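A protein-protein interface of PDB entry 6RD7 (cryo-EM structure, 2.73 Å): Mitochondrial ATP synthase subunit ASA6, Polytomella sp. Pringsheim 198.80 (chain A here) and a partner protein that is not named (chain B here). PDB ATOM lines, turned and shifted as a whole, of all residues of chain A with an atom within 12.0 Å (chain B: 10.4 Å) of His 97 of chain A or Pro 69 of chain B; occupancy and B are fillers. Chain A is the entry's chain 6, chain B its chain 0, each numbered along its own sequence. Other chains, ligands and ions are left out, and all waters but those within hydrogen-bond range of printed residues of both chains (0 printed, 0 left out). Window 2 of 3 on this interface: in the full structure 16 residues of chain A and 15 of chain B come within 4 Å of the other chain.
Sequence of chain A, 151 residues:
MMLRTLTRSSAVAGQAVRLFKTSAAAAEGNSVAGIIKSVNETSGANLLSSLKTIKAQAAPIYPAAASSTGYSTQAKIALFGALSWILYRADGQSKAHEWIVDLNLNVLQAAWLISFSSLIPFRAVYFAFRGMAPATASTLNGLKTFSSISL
The backbone carbonyl oxygen (O) of Met 71 of chain B sits at hydrogen-bond distance from the backbone NH (N) of Thr 63 of chain B (3.0 Å).
OG1 of Thr 63 of chain B sits close to N of Lys 72 of chain B, 3.5 Å away.
OG of Ser 94 of chain A is in hydrogen-bond range of O of Ala 90 of chain A, at 3.4 Å.
The side-chain hydroxyl of Ser 94 of chain A lies within hydrogen-bond range of the backbone carbonyl oxygen of Asp 91 of chain A, 2.9 Å away.
The side-chain amino group of Lys 95 of chain A lies within salt-bridge range of the side-chain carboxylate of Asp 91 of chain A, 2.5 Å away.
Of the 12 printed residues of chain B, 6 touch a printed residue of chain A.
Printed residues of chain B that touch a printed residue of chain A: Pro 62, Thr 63, Ala 64, Phe 65, Pro 66 and Pro 69.
Of the 17 printed residues of chain A, 5 touch a printed residue of chain B.
Hydrophobic or aromatic side chains of chain A that line the printed part of chain B: His 97, Trp 99 and Leu 103.
Printed residues of chain B within 4 Å of Ser 94 of chain A: Ala 64 (2.8 Å) and Phe 65 (3.8 Å).
Of chain B, only Pro 69 comes within 4 Å of His 97 of chain A.
No residue of chain B comes within 4 Å of Glu 98 of chain A.
Ile 100 of chain A touches none of the printed residues of chain B.
Printed residues of chain A within 4 Å of Thr 63 of chain B: Lys 95 (3.98 Å).
Printed residues of chain A within 4 Å of Pro 69 of chain B: His 97 (3.9 Å).
No residue of chain A comes within 4 Å of Gly 70 of chain B.
No residue of chain A comes within 4 Å of Met 71 of chain B.
The nearest residue of chain B that does not touch His 97 of chain A is Gly 70 of chain B (5.3 Å).
The nearest residue of chain A that does not touch Pro 69 of chain B is Trp 99 of chain A (5.3 Å).
Among the printed residues, pairs that only touch across the chains: Ser 94 of chain A with Phe 65 of chain B, Lys 95 of chain A with Pro 62 of chain B, Lys 95 of chain A with Thr 63 of chain B, Lys 95 of chain A with Ala 64 of chain B, His 97 of chain A with Pro 69 of chain B, Trp 99 of chain A with Pro 66 of chain B and Leu 103 of chain A with Phe 65 of chain B.
The backbone carbonyl oxygen (O) of Ala 64 of chain B sits close to the side-chain hydroxyl (OG) of Ser 94 of chain A, 3.4 Å away.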
ATOM      1  N   ARG A  89      20.495   3.616  20.714  1.00  0.00           N
ATOM      2  CA  ARG A  89      19.970   2.571  19.849  1.00  0.00           C
ATOM      3  C   ARG A  89      18.547   2.193  20.232  1.00  0.00           C
ATOM      4  O   ARG A  89      17.729   1.897  19.361  1.00  0.00           O
ATOM      5  CB  ARG A  89      20.879   1.352  19.906  1.00  0.00           C
ATOM      6  CG  ARG A  89      22.149   1.482  19.099  1.00  0.00           C
ATOM      7  CD  ARG A  89      21.874   1.579  17.630  1.00  0.00           C
ATOM      8  NE  ARG A  89      21.303   0.345  17.116  1.00  0.00           N
ATOM      9  CZ  ARG A  89      21.203   0.060  15.826  1.00  0.00           C
ATOM     10  NH1 ARG A  89      20.666  -1.085  15.440  1.00  0.00           N
ATOM     11  NH2 ARG A  89      21.641   0.924  14.924  1.00  0.00           N
ATOM     12  N   ALA A  90      18.226   2.214  21.528  1.00  0.00           N
ATOM     13  CA  ALA A  90      16.860   1.927  21.951  1.00  0.00           C
ATOM     14  C   ALA A  90      15.916   3.058  21.569  1.00  0.00           C
ATOM     15  O   ALA A  90      14.752   2.813  21.228  1.00  0.00           O
ATOM     16  CB  ALA A  90      16.818   1.678  23.455  1.00  0.00           C
ATOM     17  N   ASP A  91      16.403   4.301  21.607  1.00  0.00           N
ATOM     18  CA  ASP A  91      15.596   5.423  21.147  1.00  0.00           C
ATOM     19  C   ASP A  91      15.368   5.360  19.643  1.00  0.00           C
ATOM     20  O   ASP A  91      14.280   5.693  19.162  1.00  0.00           O
ATOM     21  CB  ASP A  91      16.265   6.738  21.534  1.00  0.00           C
ATOM     22  CG  ASP A  91      15.530   7.942  20.998  1.00  0.00           C
ATOM     23  OD1 ASP A  91      16.097   8.650  20.141  1.00  0.00           O
ATOM     24  OD2 ASP A  91      14.385   8.181  21.432  1.00  0.00           O
ATOM     25  N   GLY A  92      16.374   4.928  18.884  1.00  0.00           N
ATOM     26  CA  GLY A  92      16.177   4.758  17.453  1.00  0.00           C
ATOM     27  C   GLY A  92      15.298   3.567  17.117  1.00  0.00           C
ATOM     28  O   GLY A  92      14.605   3.565  16.099  1.00  0.00           O
ATOM     29  N   GLN A  93      15.324   2.536  17.964  1.00  0.00           N
ATOM     30  CA  GLN A  93      14.481   1.366  17.745  1.00  0.00           C
ATOM     31  C   GLN A  93      13.027   1.675  18.052  1.00  0.00           C
ATOM     32  O   GLN A  93      12.120   1.131  17.416  1.00  0.00           O
ATOM     33  CB  GLN A  93      14.954   0.204  18.614  1.00  0.00           C
ATOM     34  CG  GLN A  93      16.045  -0.640  18.007  1.00  0.00           C
ATOM     35  CD  GLN A  93      16.454  -1.770  18.918  1.00  0.00           C
ATOM     36  OE1 GLN A  93      16.096  -1.792  20.092  1.00  0.00           O
ATOM     37  NE2 GLN A  93      17.211  -2.714  18.383  1.00  0.00           N
ATOM     38  N   SER A  94      12.787   2.533  19.042  1.00  0.00           N
ATOM     39  CA  SER A  94      11.418   2.882  19.395  1.00  0.00           C
ATOM     40  C   SER A  94      10.795   3.797  18.344  1.00  0.00           C
ATOM     41  O   SER A  94       9.595   3.721  18.073  1.00  0.00           O
ATOM     42  CB  SER A  94      11.396   3.524  20.778  1.00  0.00           C
ATOM     43  OG  SER A  94      12.052   4.776  20.763  1.00  0.00           O
ATOM     44  N   LYS A  95      11.596   4.647  17.709  1.00  0.00           N
ATOM     45  CA  LYS A  95      11.043   5.512  16.676  1.00  0.00           C
ATOM     46  C   LYS A  95      10.836   4.799  15.345  1.00  0.00           C
ATOM     47  O   LYS A  95      10.299   5.410  14.416  1.00  0.00           O
ATOM     48  CB  LYS A  95      11.943   6.727  16.477  1.00  0.00           C
ATOM     49  CG  LYS A  95      11.950   7.674  17.654  1.00  0.00           C
ATOM     50  CD  LYS A  95      12.942   8.794  17.448  1.00  0.00           C
ATOM     51  CE  LYS A  95      12.761   9.872  18.493  1.00  0.00           C
ATOM     52  NZ  LYS A  95      12.762   9.296  19.857  1.00  0.00           N
ATOM     53  N   ALA A  96      11.235   3.535  15.226  1.00  0.00           N
ATOM     54  CA  ALA A  96      11.094   2.807  13.977  1.00  0.00           C
ATOM     55  C   ALA A  96       9.638   2.409  13.747  1.00  0.00           C
ATOM     56  O   ALA A  96       8.779   2.558  14.619  1.00  0.00           O
ATOM     57  CB  ALA A  96      11.985   1.568  13.977  1.00  0.00           C
ATOM     58  N   HIS A  97       9.371   1.884  12.548  1.00  0.00           N
ATOM     59  CA  HIS A  97       7.998   1.578  12.158  1.00  0.00           C
ATOM     60  C   HIS A  97       7.458   0.372  12.916  1.00  0.00           C
ATOM     61  O   HIS A  97       6.428   0.467  13.591  1.00  0.00           O
ATOM     62  CB  HIS A  97       7.910   1.344  10.653  1.00  0.00           C
ATOM     63  CG  HIS A  97       6.649   0.657  10.232  1.00  0.00           C
ATOM     64  ND1 HIS A  97       5.416   1.265  10.301  1.00  0.00           N
ATOM     65  CD2 HIS A  97       6.429  -0.588   9.751  1.00  0.00           C
ATOM     66  CE1 HIS A  97       4.489   0.425   9.878  1.00  0.00           C
ATOM     67  NE2 HIS A  97       5.078  -0.706   9.538  1.00  0.00           N
ATOM     68  N   GLU A  98       8.118  -0.775  12.803  1.00  0.00           N
ATOM     69  CA  GLU A  98       7.786  -1.918  13.651  1.00  0.00           C
ATOM     70  C   GLU A  98       8.678  -1.925  14.889  1.00  0.00           C
ATOM     71  O   GLU A  98       9.582  -2.733  15.069  1.00  0.00           O
ATOM     72  CB  GLU A  98       7.864  -3.225  12.863  1.00  0.00           C
ATOM     73  CG  GLU A  98       9.075  -3.418  11.971  1.00  0.00           C
ATOM     74  CD  GLU A  98       8.869  -4.549  10.984  1.00  0.00           C
ATOM     75  OE1 GLU A  98       7.848  -4.532  10.266  1.00  0.00           O
ATOM     76  OE2 GLU A  98       9.714  -5.466  10.939  1.00  0.00           O
ATOM     77  N   TRP A  99       8.365  -0.967  15.756  1.00  0.00           N
ATOM     78  CA  TRP A  99       9.193  -0.658  16.915  1.00  0.00           C
ATOM     79  C   TRP A  99       9.078  -1.728  17.988  1.00  0.00           C
ATOM     80  O   TRP A  99      10.074  -2.086  18.627  1.00  0.00           O
ATOM     81  CB  TRP A  99       8.777   0.698  17.474  1.00  0.00           C
ATOM     82  CG  TRP A  99       7.286   0.877  17.574  1.00  0.00           C
ATOM     83  CD1 TRP A  99       6.439   1.302  16.593  1.00  0.00           C
ATOM     84  CD2 TRP A  99       6.473   0.635  18.724  1.00  0.00           C
ATOM     85  NE1 TRP A  99       5.152   1.319  17.053  1.00  0.00           N
ATOM     86  CE2 TRP A  99       5.146   0.920  18.362  1.00  0.00           C
ATOM     87  CE3 TRP A  99       6.739   0.208  20.025  1.00  0.00           C
ATOM     88  CZ2 TRP A  99       4.091   0.790  19.251  1.00  0.00           C
ATOM     89  CZ3 TRP A  99       5.691   0.074  20.900  1.00  0.00           C
ATOM     90  CH2 TRP A  99       4.383   0.361  20.510  1.00  0.00           C
ATOM     91  N   ILE A 100       7.865  -2.237  18.211  1.00  0.00           N
ATOM     92  CA  ILE A 100       7.646  -3.250  19.230  1.00  0.00           C
ATOM     93  C   ILE A 100       8.295  -4.562  18.814  1.00  0.00           C
ATOM     94  O   ILE A 100       8.801  -5.302  19.666  1.00  0.00           O
ATOM     95  CB  ILE A 100       6.129  -3.355  19.506  1.00  0.00           C
ATOM     96  CG1 ILE A 100       5.820  -4.342  20.629  1.00  0.00           C
ATOM     97  CG2 ILE A 100       5.341  -3.671  18.247  1.00  0.00           C
ATOM     98  CD1 ILE A 100       6.026  -3.778  22.010  1.00  0.00           C
ATOM     99  N   VAL A 101       8.373  -4.813  17.509  1.00  0.00           N
ATOM    100  CA  VAL A 101       9.099  -5.948  16.959  1.00  0.00           C
ATOM    101  C   VAL A 101      10.581  -5.872  17.312  1.00  0.00           C
ATOM    102  O   VAL A 101      11.164  -6.855  17.778  1.00  0.00           O
ATOM    103  CB  VAL A 101       8.853  -5.993  15.442  1.00  0.00           C
ATOM    104  CG1 VAL A 101       9.856  -6.867  14.737  1.00  0.00           C
ATOM    105  CG2 VAL A 101       7.438  -6.468  15.172  1.00  0.00           C
ATOM    106  N   ASP A 102      11.190  -4.692  17.164  1.00  0.00           N
ATOM    107  CA  ASP A 102      12.587  -4.496  17.542  1.00  0.00           C
ATOM    108  C   ASP A 102      12.802  -4.618  19.047  1.00  0.00           C
ATOM    109  O   ASP A 102      13.795  -5.221  19.491  1.00  0.00           O
ATOM    110  CB  ASP A 102      13.056  -3.125  17.064  1.00  0.00           C
ATOM    111  CG  ASP A 102      12.889  -2.941  15.572  1.00  0.00           C
ATOM    112  OD1 ASP A 102      12.296  -3.824  14.925  1.00  0.00           O
ATOM    113  OD2 ASP A 102      13.348  -1.909  15.042  1.00  0.00           O
ATOM    114  N   LEU A 103      11.886  -4.060  19.842  1.00  0.00           N
ATOM    115  CA  LEU A 103      12.020  -4.125  21.290  1.00  0.00           C
ATOM    116  C   LEU A 103      11.871  -5.543  21.824  1.00  0.00           C
ATOM    117  O   LEU A 103      12.439  -5.862  22.872  1.00  0.00           O
ATOM    118  CB  LEU A 103      11.001  -3.205  21.957  1.00  0.00           C
ATOM    119  CG  LEU A 103      11.187  -1.709  21.721  1.00  0.00           C
ATOM    120  CD1 LEU A 103      10.161  -0.941  22.516  1.00  0.00           C
ATOM    121  CD2 LEU A 103      12.590  -1.258  22.079  1.00  0.00           C
ATOM    122  N   ASN A 104      11.131  -6.406  21.131  1.00  0.00           N
ATOM    123  CA  ASN A 104      11.115  -7.808  21.524  1.00  0.00           C
ATOM    124  C   ASN A 104      12.234  -8.625  20.891  1.00  0.00           C
ATOM    125  O   ASN A 104      12.582  -9.687  21.424  1.00  0.00           O
ATOM    126  CB  ASN A 104       9.759  -8.441  21.223  1.00  0.00           C
ATOM    127  CG  ASN A 104       8.662  -7.854  22.069  1.00  0.00           C
ATOM    128  OD1 ASN A 104       7.851  -7.063  21.608  1.00  0.00           O
ATOM    129  ND2 ASN A 104       8.668  -8.197  23.342  1.00  0.00           N
ATOM    130  N   LEU A 105      12.831  -8.148  19.796  1.00  0.00           N
ATOM    131  CA  LEU A 105      14.081  -8.741  19.332  1.00  0.00           C
ATOM    132  C   LEU A 105      15.203  -8.571  20.343  1.00  0.00           C
ATOM    133  O   LEU A 105      16.052  -9.463  20.476  1.00  0.00           O
ATOM    134  CB  LEU A 105      14.522  -8.123  18.012  1.00  0.00           C
ATOM    135  CG  LEU A 105      13.802  -8.499  16.729  1.00  0.00           C
ATOM    136  CD1 LEU A 105      14.691  -8.120  15.588  1.00  0.00           C
ATOM    137  CD2 LEU A 105      13.489  -9.965  16.701  1.00  0.00           C
ATOM    138  N   ASP B  59       8.160  13.764   8.727  1.00  0.00           N
ATOM    139  CA  ASP B  59       8.753  12.447   8.504  1.00  0.00           C
ATOM    140  C   ASP B  59      10.057  12.284   9.273  1.00  0.00           C
ATOM    141  O   ASP B  59      10.424  11.167   9.652  1.00  0.00           O
ATOM    142  CB  ASP B  59       8.987  12.214   7.014  1.00  0.00           C
ATOM    143  CG  ASP B  59       7.893  11.390   6.375  1.00  0.00           C
ATOM    144  OD1 ASP B  59       6.870  11.142   7.045  1.00  0.00           O
ATOM    145  OD2 ASP B  59       8.055  10.987   5.204  1.00  0.00           O
ATOM    146  N   PRO B  62       9.533  11.117  14.020  1.00  0.00           N
ATOM    147  CA  PRO B  62       8.536  10.104  14.368  1.00  0.00           C
ATOM    148  C   PRO B  62       8.349   9.986  15.870  1.00  0.00           C
ATOM    149  O   PRO B  62       9.238  10.297  16.665  1.00  0.00           O
ATOM    150  CB  PRO B  62       9.125   8.820  13.778  1.00  0.00           C
ATOM    151  CG  PRO B  62      10.576   9.029  13.848  1.00  0.00           C
ATOM    152  CD  PRO B  62      10.840  10.501  13.728  1.00  0.00           C
ATOM    153  N   THR B  63       7.162   9.527  16.252  1.00  0.00           N
ATOM    154  CA  THR B  63       6.785   9.446  17.655  1.00  0.00           C
ATOM    155  C   THR B  63       7.477   8.258  18.313  1.00  0.00           C
ATOM    156  O   THR B  63       7.589   7.184  17.716  1.00  0.00           O
ATOM    157  CB  THR B  63       5.261   9.343  17.766  1.00  0.00           C
ATOM    158  OG1 THR B  63       4.680  10.560  17.285  1.00  0.00           O
ATOM    159  CG2 THR B  63       4.792   9.130  19.196  1.00  0.00           C
ATOM    160  N   ALA B  64       7.976   8.478  19.535  1.00  0.00           N
ATOM    161  CA  ALA B  64       8.760   7.522  20.309  1.00  0.00           C
ATOM    162  C   ALA B  64       8.079   6.179  20.522  1.00  0.00           C
ATOM    163  O   ALA B  64       8.680   5.142  20.267  1.00  0.00           O
ATOM    164  CB  ALA B  64       9.121   8.123  21.666  1.00  0.00           C
ATOM    165  N   PHE B  65       6.847   6.150  21.012  1.00  0.00           N
ATOM    166  CA  PHE B  65       6.119   4.894  21.167  1.00  0.00           C
ATOM    167  C   PHE B  65       4.737   5.117  20.572  1.00  0.00           C
ATOM    168  O   PHE B  65       3.767   5.353  21.308  1.00  0.00           O
ATOM    169  CB  PHE B  65       6.054   4.446  22.624  1.00  0.00           C
ATOM    170  CG  PHE B  65       7.376   3.995  23.178  1.00  0.00           C
ATOM    171  CD1 PHE B  65       7.710   2.654  23.201  1.00  0.00           C
ATOM    172  CD2 PHE B  65       8.282   4.913  23.684  1.00  0.00           C
ATOM    173  CE1 PHE B  65       8.924   2.239  23.710  1.00  0.00           C
ATOM    174  CE2 PHE B  65       9.497   4.501  24.191  1.00  0.00           C
ATOM    175  CZ  PHE B  65       9.816   3.164  24.205  1.00  0.00           C
ATOM    176  N   PRO B  66       4.612   5.055  19.248  1.00  0.00           N
ATOM    177  CA  PRO B  66       3.399   5.558  18.599  1.00  0.00           C
ATOM    178  C   PRO B  66       2.224   4.616  18.796  1.00  0.00           C
ATOM    179  O   PRO B  66       2.329   3.406  18.590  1.00  0.00           O
ATOM    180  CB  PRO B  66       3.807   5.669  17.127  1.00  0.00           C
ATOM    181  CG  PRO B  66       4.882   4.682  16.958  1.00  0.00           C
ATOM    182  CD  PRO B  66       5.588   4.540  18.273  1.00  0.00           C
ATOM    183  N   LYS B  67       1.099   5.189  19.221  1.00  0.00           N
ATOM    184  CA  LYS B  67      -0.105   4.396  19.418  1.00  0.00           C
ATOM    185  C   LYS B  67      -0.693   3.960  18.086  1.00  0.00           C
ATOM    186  O   LYS B  67      -1.411   2.960  18.016  1.00  0.00           O
ATOM    187  CB  LYS B  67      -1.124   5.192  20.225  1.00  0.00           C
ATOM    188  CG  LYS B  67      -0.630   5.585  21.595  1.00  0.00           C
ATOM    189  CD  LYS B  67      -0.526   4.380  22.494  1.00  0.00           C
ATOM    190  CE  LYS B  67       0.166   4.734  23.787  1.00  0.00           C
ATOM    191  NZ  LYS B  67       0.163   3.592  24.729  1.00  0.00           N
ATOM    192  N   VAL B  68      -0.412   4.703  17.024  1.00  0.00           N
ATOM    193  CA  VAL B  68      -0.767   4.303  15.667  1.00  0.00           C
ATOM    194  C   VAL B  68       0.512   4.367  14.840  1.00  0.00           C
ATOM    195  O   VAL B  68       1.256   5.352  14.949  1.00  0.00           O
ATOM    196  CB  VAL B  68      -1.880   5.196  15.093  1.00  0.00           C
ATOM    197  CG1 VAL B  68      -2.065   4.948  13.610  1.00  0.00           C
ATOM    198  CG2 VAL B  68      -3.184   4.952  15.826  1.00  0.00           C
ATOM    199  N   PRO B  69       0.831   3.339  14.049  1.00  0.00           N
ATOM    200  CA  PRO B  69       2.055   3.366  13.232  1.00  0.00           C
ATOM    201  C   PRO B  69       2.006   4.451  12.168  1.00  0.00           C
ATOM    202  O   PRO B  69       1.184   4.414  11.252  1.00  0.00           O
ATOM    203  CB  PRO B  69       2.088   1.969  12.608  1.00  0.00           C
ATOM    204  CG  PRO B  69       1.241   1.136  13.490  1.00  0.00           C
ATOM    205  CD  PRO B  69       0.167   2.028  13.996  1.00  0.00           C
ATOM    206  N   GLY B  70       2.903   5.421  12.300  1.00  0.00           N
ATOM    207  CA  GLY B  70       2.919   6.591  11.441  1.00  0.00           C
ATOM    208  C   GLY B  70       2.725   7.897  12.175  1.00  0.00           C
ATOM    209  O   GLY B  70       2.699   8.951  11.525  1.00  0.00           O
ATOM    210  N   MET B  71       2.575   7.872  13.498  1.00  0.00           N
ATOM    211  CA  MET B  71       2.448   9.094  14.277  1.00  0.00           C
ATOM    212  C   MET B  71       3.752   9.873  14.256  1.00  0.00           C
ATOM    213  O   MET B  71       4.835   9.306  14.421  1.00  0.00           O
ATOM    214  CB  MET B  71       2.074   8.772  15.721  1.00  0.00           C
ATOM    215  CG  MET B  71       0.616   8.468  15.936  1.00  0.00           C
ATOM    216  SD  MET B  71       0.195   8.243  17.670  1.00  0.00           S
ATOM    217  CE  MET B  71       1.101   9.593  18.414  1.00  0.00           C
ATOM    218  N   LYS B  72       3.645  11.178  14.044  1.00  0.00           N
ATOM    219  CA  LYS B  72       4.803  12.052  13.968  1.00  0.00           C
ATOM    220  C   LYS B  72       4.743  13.068  15.098  1.00  0.00           C
ATOM    221  O   LYS B  72       3.658  13.426  15.565  1.00  0.00           O
ATOM    222  CB  LYS B  72       4.870  12.753  12.613  1.00  0.00           C
ATOM    223  CG  LYS B  72       4.748  11.807  11.426  1.00  0.00           C
ATOM    224  CD  LYS B  72       5.783  10.692  11.480  1.00  0.00           C
ATOM    225  CE  LYS B  72       6.001  10.072  10.116  1.00  0.00           C
ATOM    226  NZ  LYS B  72       7.047   9.016  10.162  1.00  0.00           N
